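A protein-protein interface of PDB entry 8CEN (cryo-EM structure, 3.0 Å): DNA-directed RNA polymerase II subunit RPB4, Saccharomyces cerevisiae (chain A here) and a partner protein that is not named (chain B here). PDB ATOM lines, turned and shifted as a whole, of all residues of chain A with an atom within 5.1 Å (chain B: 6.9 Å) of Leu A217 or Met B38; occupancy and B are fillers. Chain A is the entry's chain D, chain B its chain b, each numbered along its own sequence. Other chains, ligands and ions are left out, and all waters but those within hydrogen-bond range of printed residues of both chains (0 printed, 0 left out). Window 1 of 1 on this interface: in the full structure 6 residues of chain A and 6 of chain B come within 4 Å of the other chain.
The backbone carbonyl oxygen of Asn A216 is in hydrogen-bond range of the guanidinium group of Arg B39, 2.8 Å away.
Thr A159 touches Gln B42 (CG2 to NE2, 3.4 Å). Gln B31 touches Glu A213. Leu A217 touches Met B38 (CD2 to CE, 3.6 Å). CD2 of Leu A217 touches NH1 of Arg B39 (3.4 Å).
Leu A217 touches just these residues of chain B: Met B38 (3.6 Å) and Arg B39 (3.4 Å). Met B38 touches just one residue of chain A: Leu A217. Printed residues of chain B within 4 Å of Thr A159: Gln B42 (3.4 Å). Of the printed residues of chain A, Gln B42 touches Thr A159. Of the printed residues of chain A, Gln B31 touches Glu A213 (3.96 Å). Of the printed residues of chain B, Asn A216 touches Arg B39. Of the printed residues of chain A, Arg B39 touches Asn A216 and Leu A217.
Of the 14 printed residues of chain B, 4 touch a printed residue of chain A. Of the 12 printed residues of chain A, 4 touch a printed residue of chain B. Hydrophobic or aromatic side chains of chain A within 4 Å of the printed part of chain B: Leu A217. Along chain A the printed residues that touch a printed residue of chain B span positions 159 to 217.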
ATOM      1  N   ARG A 153      31.479  -7.143  31.498  1.00  0.00           N
ATOM      2  CA  ARG A 153      30.763  -7.391  30.253  1.00  0.00           C
ATOM      3  C   ARG A 153      30.288  -6.101  29.599  1.00  0.00           C
ATOM      4  O   ARG A 153      30.220  -6.021  28.367  1.00  0.00           O
ATOM      5  CB  ARG A 153      29.576  -8.320  30.506  1.00  0.00           C
ATOM      6  CG  ARG A 153      29.905  -9.798  30.372  1.00  0.00           C
ATOM      7  CD  ARG A 153      28.661 -10.657  30.511  1.00  0.00           C
ATOM      8  NE  ARG A 153      27.817 -10.575  29.325  1.00  0.00           N
ATOM      9  CZ  ARG A 153      26.767 -11.351  29.095  1.00  0.00           C
ATOM     10  NH1 ARG A 153      26.399 -12.289  29.952  1.00  0.00           N
ATOM     11  NH2 ARG A 153      26.069 -11.183  27.975  1.00  0.00           N
ATOM     12  N   PHE A 154      29.957  -5.087  30.394  1.00  0.00           N
ATOM     13  CA  PHE A 154      29.379  -3.854  29.886  1.00  0.00           C
ATOM     14  C   PHE A 154      30.204  -2.664  30.349  1.00  0.00           C
ATOM     15  O   PHE A 154      30.760  -2.660  31.451  1.00  0.00           O
ATOM     16  CB  PHE A 154      27.922  -3.719  30.336  1.00  0.00           C
ATOM     17  CG  PHE A 154      27.136  -4.991  30.194  1.00  0.00           C
ATOM     18  CD1 PHE A 154      26.761  -5.449  28.941  1.00  0.00           C
ATOM     19  CD2 PHE A 154      26.803  -5.746  31.306  1.00  0.00           C
ATOM     20  CE1 PHE A 154      26.048  -6.625  28.802  1.00  0.00           C
ATOM     21  CE2 PHE A 154      26.093  -6.926  31.174  1.00  0.00           C
ATOM     22  CZ  PHE A 154      25.715  -7.365  29.920  1.00  0.00           C
ATOM     23  N   THR A 159      24.225   1.238  29.498  1.00  0.00           N
ATOM     24  CA  THR A 159      24.141  -0.168  29.113  1.00  0.00           C
ATOM     25  C   THR A 159      23.927  -1.066  30.326  1.00  0.00           C
ATOM     26  O   THR A 159      23.102  -1.991  30.279  1.00  0.00           O
ATOM     27  CB  THR A 159      25.396  -0.599  28.354  1.00  0.00           C
ATOM     28  OG1 THR A 159      26.556  -0.055  28.994  1.00  0.00           O
ATOM     29  CG2 THR A 159      25.339  -0.117  26.911  1.00  0.00           C
ATOM     30  N   ALA A 162      20.449  -0.662  31.556  1.00  0.00           N
ATOM     31  CA  ALA A 162      19.605  -1.435  30.655  1.00  0.00           C
ATOM     32  C   ALA A 162      19.594  -2.906  31.047  1.00  0.00           C
ATOM     33  O   ALA A 162      18.549  -3.560  30.982  1.00  0.00           O
ATOM     34  CB  ALA A 162      20.074  -1.262  29.211  1.00  0.00           C
ATOM     35  N   VAL A 163      20.744  -3.439  31.475  1.00  0.00           N
ATOM     36  CA  VAL A 163      20.779  -4.834  31.927  1.00  0.00           C
ATOM     37  C   VAL A 163      19.955  -5.028  33.205  1.00  0.00           C
ATOM     38  O   VAL A 163      19.194  -6.000  33.316  1.00  0.00           O
ATOM     39  CB  VAL A 163      22.232  -5.319  32.095  1.00  0.00           C
ATOM     40  CG1 VAL A 163      22.266  -6.770  32.544  1.00  0.00           C
ATOM     41  CG2 VAL A 163      22.980  -5.175  30.788  1.00  0.00           C
ATOM     42  N   GLU A 213      19.614 -10.794  23.595  1.00  0.00           N
ATOM     43  CA  GLU A 213      19.944  -9.365  23.706  1.00  0.00           C
ATOM     44  C   GLU A 213      21.031  -9.049  24.734  1.00  0.00           C
ATOM     45  O   GLU A 213      21.639  -7.982  24.625  1.00  0.00           O
ATOM     46  CB  GLU A 213      18.755  -8.410  23.965  1.00  0.00           C
ATOM     47  CG  GLU A 213      17.703  -8.203  22.840  1.00  0.00           C
ATOM     48  CD  GLU A 213      16.601  -9.220  22.744  1.00  0.00           C
ATOM     49  OE1 GLU A 213      16.543 -10.107  23.592  1.00  0.00           O
ATOM     50  OE2 GLU A 213      15.782  -9.125  21.806  1.00  0.00           O
ATOM     51  N   LEU A 214      21.338  -9.931  25.690  1.00  0.00           N
ATOM     52  CA  LEU A 214      22.567  -9.715  26.459  1.00  0.00           C
ATOM     53  C   LEU A 214      23.808  -9.890  25.586  1.00  0.00           C
ATOM     54  O   LEU A 214      24.784  -9.140  25.725  1.00  0.00           O
ATOM     55  CB  LEU A 214      22.632 -10.636  27.678  1.00  0.00           C
ATOM     56  CG  LEU A 214      21.605 -10.397  28.786  1.00  0.00           C
ATOM     57  CD1 LEU A 214      21.700 -11.469  29.859  1.00  0.00           C
ATOM     58  CD2 LEU A 214      21.796  -9.013  29.388  1.00  0.00           C
ATOM     59  N   SER A 215      23.780 -10.862  24.671  1.00  0.00           N
ATOM     60  CA  SER A 215      24.870 -11.015  23.712  1.00  0.00           C
ATOM     61  C   SER A 215      24.958  -9.813  22.780  1.00  0.00           C
ATOM     62  O   SER A 215      26.055  -9.418  22.366  1.00  0.00           O
ATOM     63  CB  SER A 215      24.685 -12.306  22.915  1.00  0.00           C
ATOM     64  OG  SER A 215      23.650 -12.169  21.956  1.00  0.00           O
ATOM     65  N   ASN A 216      23.810  -9.231  22.423  1.00  0.00           N
ATOM     66  CA  ASN A 216      23.820  -8.004  21.627  1.00  0.00           C
ATOM     67  C   ASN A 216      24.388  -6.827  22.416  1.00  0.00           C
ATOM     68  O   ASN A 216      25.142  -6.014  21.868  1.00  0.00           O
ATOM     69  CB  ASN A 216      22.412  -7.682  21.126  1.00  0.00           C
ATOM     70  CG  ASN A 216      21.806  -8.812  20.321  1.00  0.00           C
ATOM     71  OD1 ASN A 216      20.619  -9.108  20.444  1.00  0.00           O
ATOM     72  ND2 ASN A 216      22.622  -9.455  19.492  1.00  0.00           N
ATOM     73  N   LEU A 217      24.036  -6.716  23.701  1.00  0.00           N
ATOM     74  CA  LEU A 217      24.553  -5.638  24.538  1.00  0.00           C
ATOM     75  C   LEU A 217      26.024  -5.805  24.882  1.00  0.00           C
ATOM     76  O   LEU A 217      26.661  -4.825  25.284  1.00  0.00           O
ATOM     77  CB  LEU A 217      23.731  -5.523  25.826  1.00  0.00           C
ATOM     78  CG  LEU A 217      22.325  -4.947  25.663  1.00  0.00           C
ATOM     79  CD1 LEU A 217      21.759  -4.476  26.989  1.00  0.00           C
ATOM     80  CD2 LEU A 217      22.404  -3.776  24.702  1.00  0.00           C
ATOM     81  N   GLU A 218      26.560  -7.018  24.760  1.00  0.00           N
ATOM     82  CA  GLU A 218      27.998  -7.220  24.894  1.00  0.00           C
ATOM     83  C   GLU A 218      28.752  -6.398  23.856  1.00  0.00           C
ATOM     84  O   GLU A 218      28.457  -6.460  22.659  1.00  0.00           O
ATOM     85  CB  GLU A 218      28.338  -8.703  24.738  1.00  0.00           C
ATOM     86  CG  GLU A 218      29.818  -9.036  24.899  1.00  0.00           C
ATOM     87  CD  GLU A 218      30.349  -8.775  26.295  1.00  0.00           C
ATOM     88  OE1 GLU A 218      29.554  -8.809  27.257  1.00  0.00           O
ATOM     89  OE2 GLU A 218      31.568  -8.537  26.433  1.00  0.00           O
ATOM     90  N   THR A 219      29.728  -5.621  24.322  1.00  0.00           N
ATOM     91  CA  THR A 219      30.489  -4.731  23.459  1.00  0.00           C
ATOM     92  C   THR A 219      31.961  -4.785  23.840  1.00  0.00           C
ATOM     93  O   THR A 219      32.312  -5.109  24.980  1.00  0.00           O
ATOM     94  CB  THR A 219      29.961  -3.287  23.535  1.00  0.00           C
ATOM     95  OG1 THR A 219      30.693  -2.454  22.628  1.00  0.00           O
ATOM     96  CG2 THR A 219      30.080  -2.737  24.948  1.00  0.00           C
ATOM     97  N   GLN B  31      12.163  -7.741  17.948  1.00  0.00           N
ATOM     98  CA  GLN B  31      13.559  -7.745  18.369  1.00  0.00           C
ATOM     99  C   GLN B  31      14.373  -6.687  17.630  1.00  0.00           C
ATOM    100  O   GLN B  31      15.229  -6.027  18.234  1.00  0.00           O
ATOM    101  CB  GLN B  31      14.150  -9.150  18.200  1.00  0.00           C
ATOM    102  CG  GLN B  31      14.380  -9.642  16.773  1.00  0.00           C
ATOM    103  CD  GLN B  31      13.150 -10.288  16.164  1.00  0.00           C
ATOM    104  OE1 GLN B  31      12.039 -10.150  16.676  1.00  0.00           O
ATOM    105  NE2 GLN B  31      13.345 -10.997  15.056  1.00  0.00           N
ATOM    106  N   ALA B  32      14.097  -6.483  16.337  1.00  0.00           N
ATOM    107  CA  ALA B  32      14.801  -5.460  15.569  1.00  0.00           C
ATOM    108  C   ALA B  32      14.476  -4.071  16.092  1.00  0.00           C
ATOM    109  O   ALA B  32      15.367  -3.230  16.276  1.00  0.00           O
ATOM    110  CB  ALA B  32      14.431  -5.573  14.092  1.00  0.00           C
ATOM    111  N   LEU B  33      13.192  -3.824  16.351  1.00  0.00           N
ATOM    112  CA  LEU B  33      12.759  -2.527  16.847  1.00  0.00           C
ATOM    113  C   LEU B  33      13.273  -2.279  18.260  1.00  0.00           C
ATOM    114  O   LEU B  33      13.660  -1.155  18.593  1.00  0.00           O
ATOM    115  CB  LEU B  33      11.239  -2.448  16.780  1.00  0.00           C
ATOM    116  CG  LEU B  33      10.583  -1.082  16.636  1.00  0.00           C
ATOM    117  CD1 LEU B  33      10.782  -0.539  15.237  1.00  0.00           C
ATOM    118  CD2 LEU B  33       9.117  -1.241  16.923  1.00  0.00           C
ATOM    119  N   ASP B  34      13.317  -3.324  19.093  1.00  0.00           N
ATOM    120  CA  ASP B  34      13.875  -3.179  20.434  1.00  0.00           C
ATOM    121  C   ASP B  34      15.367  -2.865  20.391  1.00  0.00           C
ATOM    122  O   ASP B  34      15.844  -1.995  21.133  1.00  0.00           O
ATOM    123  CB  ASP B  34      13.621  -4.448  21.245  1.00  0.00           C
ATOM    124  CG  ASP B  34      13.371  -4.160  22.709  1.00  0.00           C
ATOM    125  OD1 ASP B  34      13.696  -3.043  23.162  1.00  0.00           O
ATOM    126  OD2 ASP B  34      12.851  -5.054  23.408  1.00  0.00           O
ATOM    127  N   ALA B  35      16.115  -3.558  19.527  1.00  0.00           N
ATOM    128  CA  ALA B  35      17.549  -3.313  19.417  1.00  0.00           C
ATOM    129  C   ALA B  35      17.832  -1.899  18.924  1.00  0.00           C
ATOM    130  O   ALA B  35      18.677  -1.187  19.490  1.00  0.00           O
ATOM    131  CB  ALA B  35      18.186  -4.349  18.490  1.00  0.00           C
ATOM    132  N   VAL B  36      17.112  -1.463  17.884  1.00  0.00           N
ATOM    133  CA  VAL B  36      17.356  -0.123  17.365  1.00  0.00           C
ATOM    134  C   VAL B  36      16.896   0.925  18.374  1.00  0.00           C
ATOM    135  O   VAL B  36      17.502   1.995  18.471  1.00  0.00           O
ATOM    136  CB  VAL B  36      16.713   0.068  15.971  1.00  0.00           C
ATOM    137  CG1 VAL B  36      15.203   0.077  16.032  1.00  0.00           C
ATOM    138  CG2 VAL B  36      17.225   1.335  15.306  1.00  0.00           C
ATOM    139  N   ARG B  37      15.888   0.611  19.201  1.00  0.00           N
ATOM    140  CA  ARG B  37      15.476   1.533  20.253  1.00  0.00           C
ATOM    141  C   ARG B  37      16.554   1.684  21.316  1.00  0.00           C
ATOM    142  O   ARG B  37      16.803   2.793  21.796  1.00  0.00           O
ATOM    143  CB  ARG B  37      14.169   1.062  20.887  1.00  0.00           C
ATOM    144  CG  ARG B  37      13.590   2.035  21.898  1.00  0.00           C
ATOM    145  CD  ARG B  37      12.693   1.340  22.901  1.00  0.00           C
ATOM    146  NE  ARG B  37      13.387   0.306  23.656  1.00  0.00           N
ATOM    147  CZ  ARG B  37      14.014   0.511  24.806  1.00  0.00           C
ATOM    148  NH1 ARG B  37      14.084   1.716  25.349  1.00  0.00           N
ATOM    149  NH2 ARG B  37      14.580  -0.516  25.429  1.00  0.00           N
ATOM    150  N   MET B  38      17.209   0.582  21.689  1.00  0.00           N
ATOM    151  CA  MET B  38      18.244   0.657  22.719  1.00  0.00           C
ATOM    152  C   MET B  38      19.475   1.422  22.229  1.00  0.00           C
ATOM    153  O   MET B  38      19.973   2.320  22.926  1.00  0.00           O
ATOM    154  CB  MET B  38      18.598  -0.753  23.199  1.00  0.00           C
ATOM    155  CG  MET B  38      17.393  -1.418  23.869  1.00  0.00           C
ATOM    156  SD  MET B  38      17.298  -3.218  23.843  1.00  0.00           S
ATOM    157  CE  MET B  38      18.833  -3.648  24.624  1.00  0.00           C
ATOM    158  N   ARG B  39      19.962   1.108  21.017  1.00  0.00           N
ATOM    159  CA  ARG B  39      21.082   1.882  20.469  1.00  0.00           C
ATOM    160  C   ARG B  39      20.704   3.343  20.230  1.00  0.00           C
ATOM    161  O   ARG B  39      21.521   4.249  20.451  1.00  0.00           O
ATOM    162  CB  ARG B  39      21.625   1.264  19.176  1.00  0.00           C
ATOM    163  CG  ARG B  39      22.521   0.026  19.314  1.00  0.00           C
ATOM    164  CD  ARG B  39      21.800  -1.292  19.415  1.00  0.00           C
ATOM    165  NE  ARG B  39      22.723  -2.415  19.308  1.00  0.00           N
ATOM    166  CZ  ARG B  39      23.283  -3.019  20.346  1.00  0.00           C
ATOM    167  NH1 ARG B  39      23.041  -2.626  21.584  1.00  0.00           N
ATOM    168  NH2 ARG B  39      24.107  -4.041  20.136  1.00  0.00           N
ATOM    169  N   LEU B  40      19.467   3.597  19.804  1.00  0.00           N
ATOM    170  CA  LEU B  40      19.041   4.959  19.519  1.00  0.00           C
ATOM    171  C   LEU B  40      18.869   5.769  20.798  1.00  0.00           C
ATOM    172  O   LEU B  40      19.158   6.970  20.815  1.00  0.00           O
ATOM    173  CB  LEU B  40      17.748   4.898  18.710  1.00  0.00           C
ATOM    174  CG  LEU B  40      17.258   6.090  17.907  1.00  0.00           C
ATOM    175  CD1 LEU B  40      18.404   6.734  17.161  1.00  0.00           C
ATOM    176  CD2 LEU B  40      16.245   5.547  16.930  1.00  0.00           C
ATOM    177  N   ALA B  41      18.427   5.122  21.881  1.00  0.00           N
ATOM    178  CA  ALA B  41      18.367   5.775  23.182  1.00  0.00           C
ATOM    179  C   ALA B  41      19.760   6.090  23.704  1.00  0.00           C
ATOM    180  O   ALA B  41      19.970   7.143  24.316  1.00  0.00           O
ATOM    181  CB  ALA B  41      17.608   4.897  24.176  1.00  0.00           C
ATOM    182  N   GLN B  42      20.720   5.184  23.477  1.00  0.00           N
ATOM    183  CA  GLN B  42      22.107   5.465  23.851  1.00  0.00           C
ATOM    184  C   GLN B  42      22.643   6.683  23.104  1.00  0.00           C
ATOM    185  O   GLN B  42      23.264   7.577  23.703  1.00  0.00           O
ATOM    186  CB  GLN B  42      22.977   4.240  23.569  1.00  0.00           C
ATOM    187  CG  GLN B  42      22.826   3.113  24.574  1.00  0.00           C
ATOM    188  CD  GLN B  42      23.554   1.855  24.142  1.00  0.00           C
ATOM    189  OE1 GLN B  42      24.586   1.920  23.478  1.00  0.00           O
ATOM    190  NE2 GLN B  42      23.013   0.700  24.514  1.00  0.00           N
ATOM    191  N   LEU B  43      22.387   6.743  21.792  1.00  0.00           N
ATOM    192  CA  LEU B  43      22.821   7.883  20.986  1.00  0.00           C
ATOM    193  C   LEU B  43      22.152   9.179  21.438  1.00  0.00           C
ATOM    194  O   LEU B  43      22.809  10.224  21.535  1.00  0.00           O
ATOM    195  CB  LEU B  43      22.529   7.618  19.509  1.00  0.00           C
ATOM    196  CG  LEU B  43      22.814   8.751  18.520  1.00  0.00           C
ATOM    197  CD1 LEU B  43      24.280   9.143  18.548  1.00  0.00           C
ATOM    198  CD2 LEU B  43      22.389   8.359  17.115  1.00  0.00           C
ATOM    199  N   VAL B  79      24.240   1.975  15.894  1.00  0.00           N
ATOM    200  CA  VAL B  79      22.839   1.970  15.486  1.00  0.00           C
ATOM    201  C   VAL B  79      22.719   1.816  13.971  1.00  0.00           C
ATOM    202  O   VAL B  79      21.801   1.141  13.485  1.00  0.00           O
ATOM    203  CB  VAL B  79      22.094   3.213  16.030  1.00  0.00           C
ATOM    204  CG1 VAL B  79      22.467   4.497  15.302  1.00  0.00           C
ATOM    205  CG2 VAL B  79      20.589   2.991  15.977  1.00  0.00           C
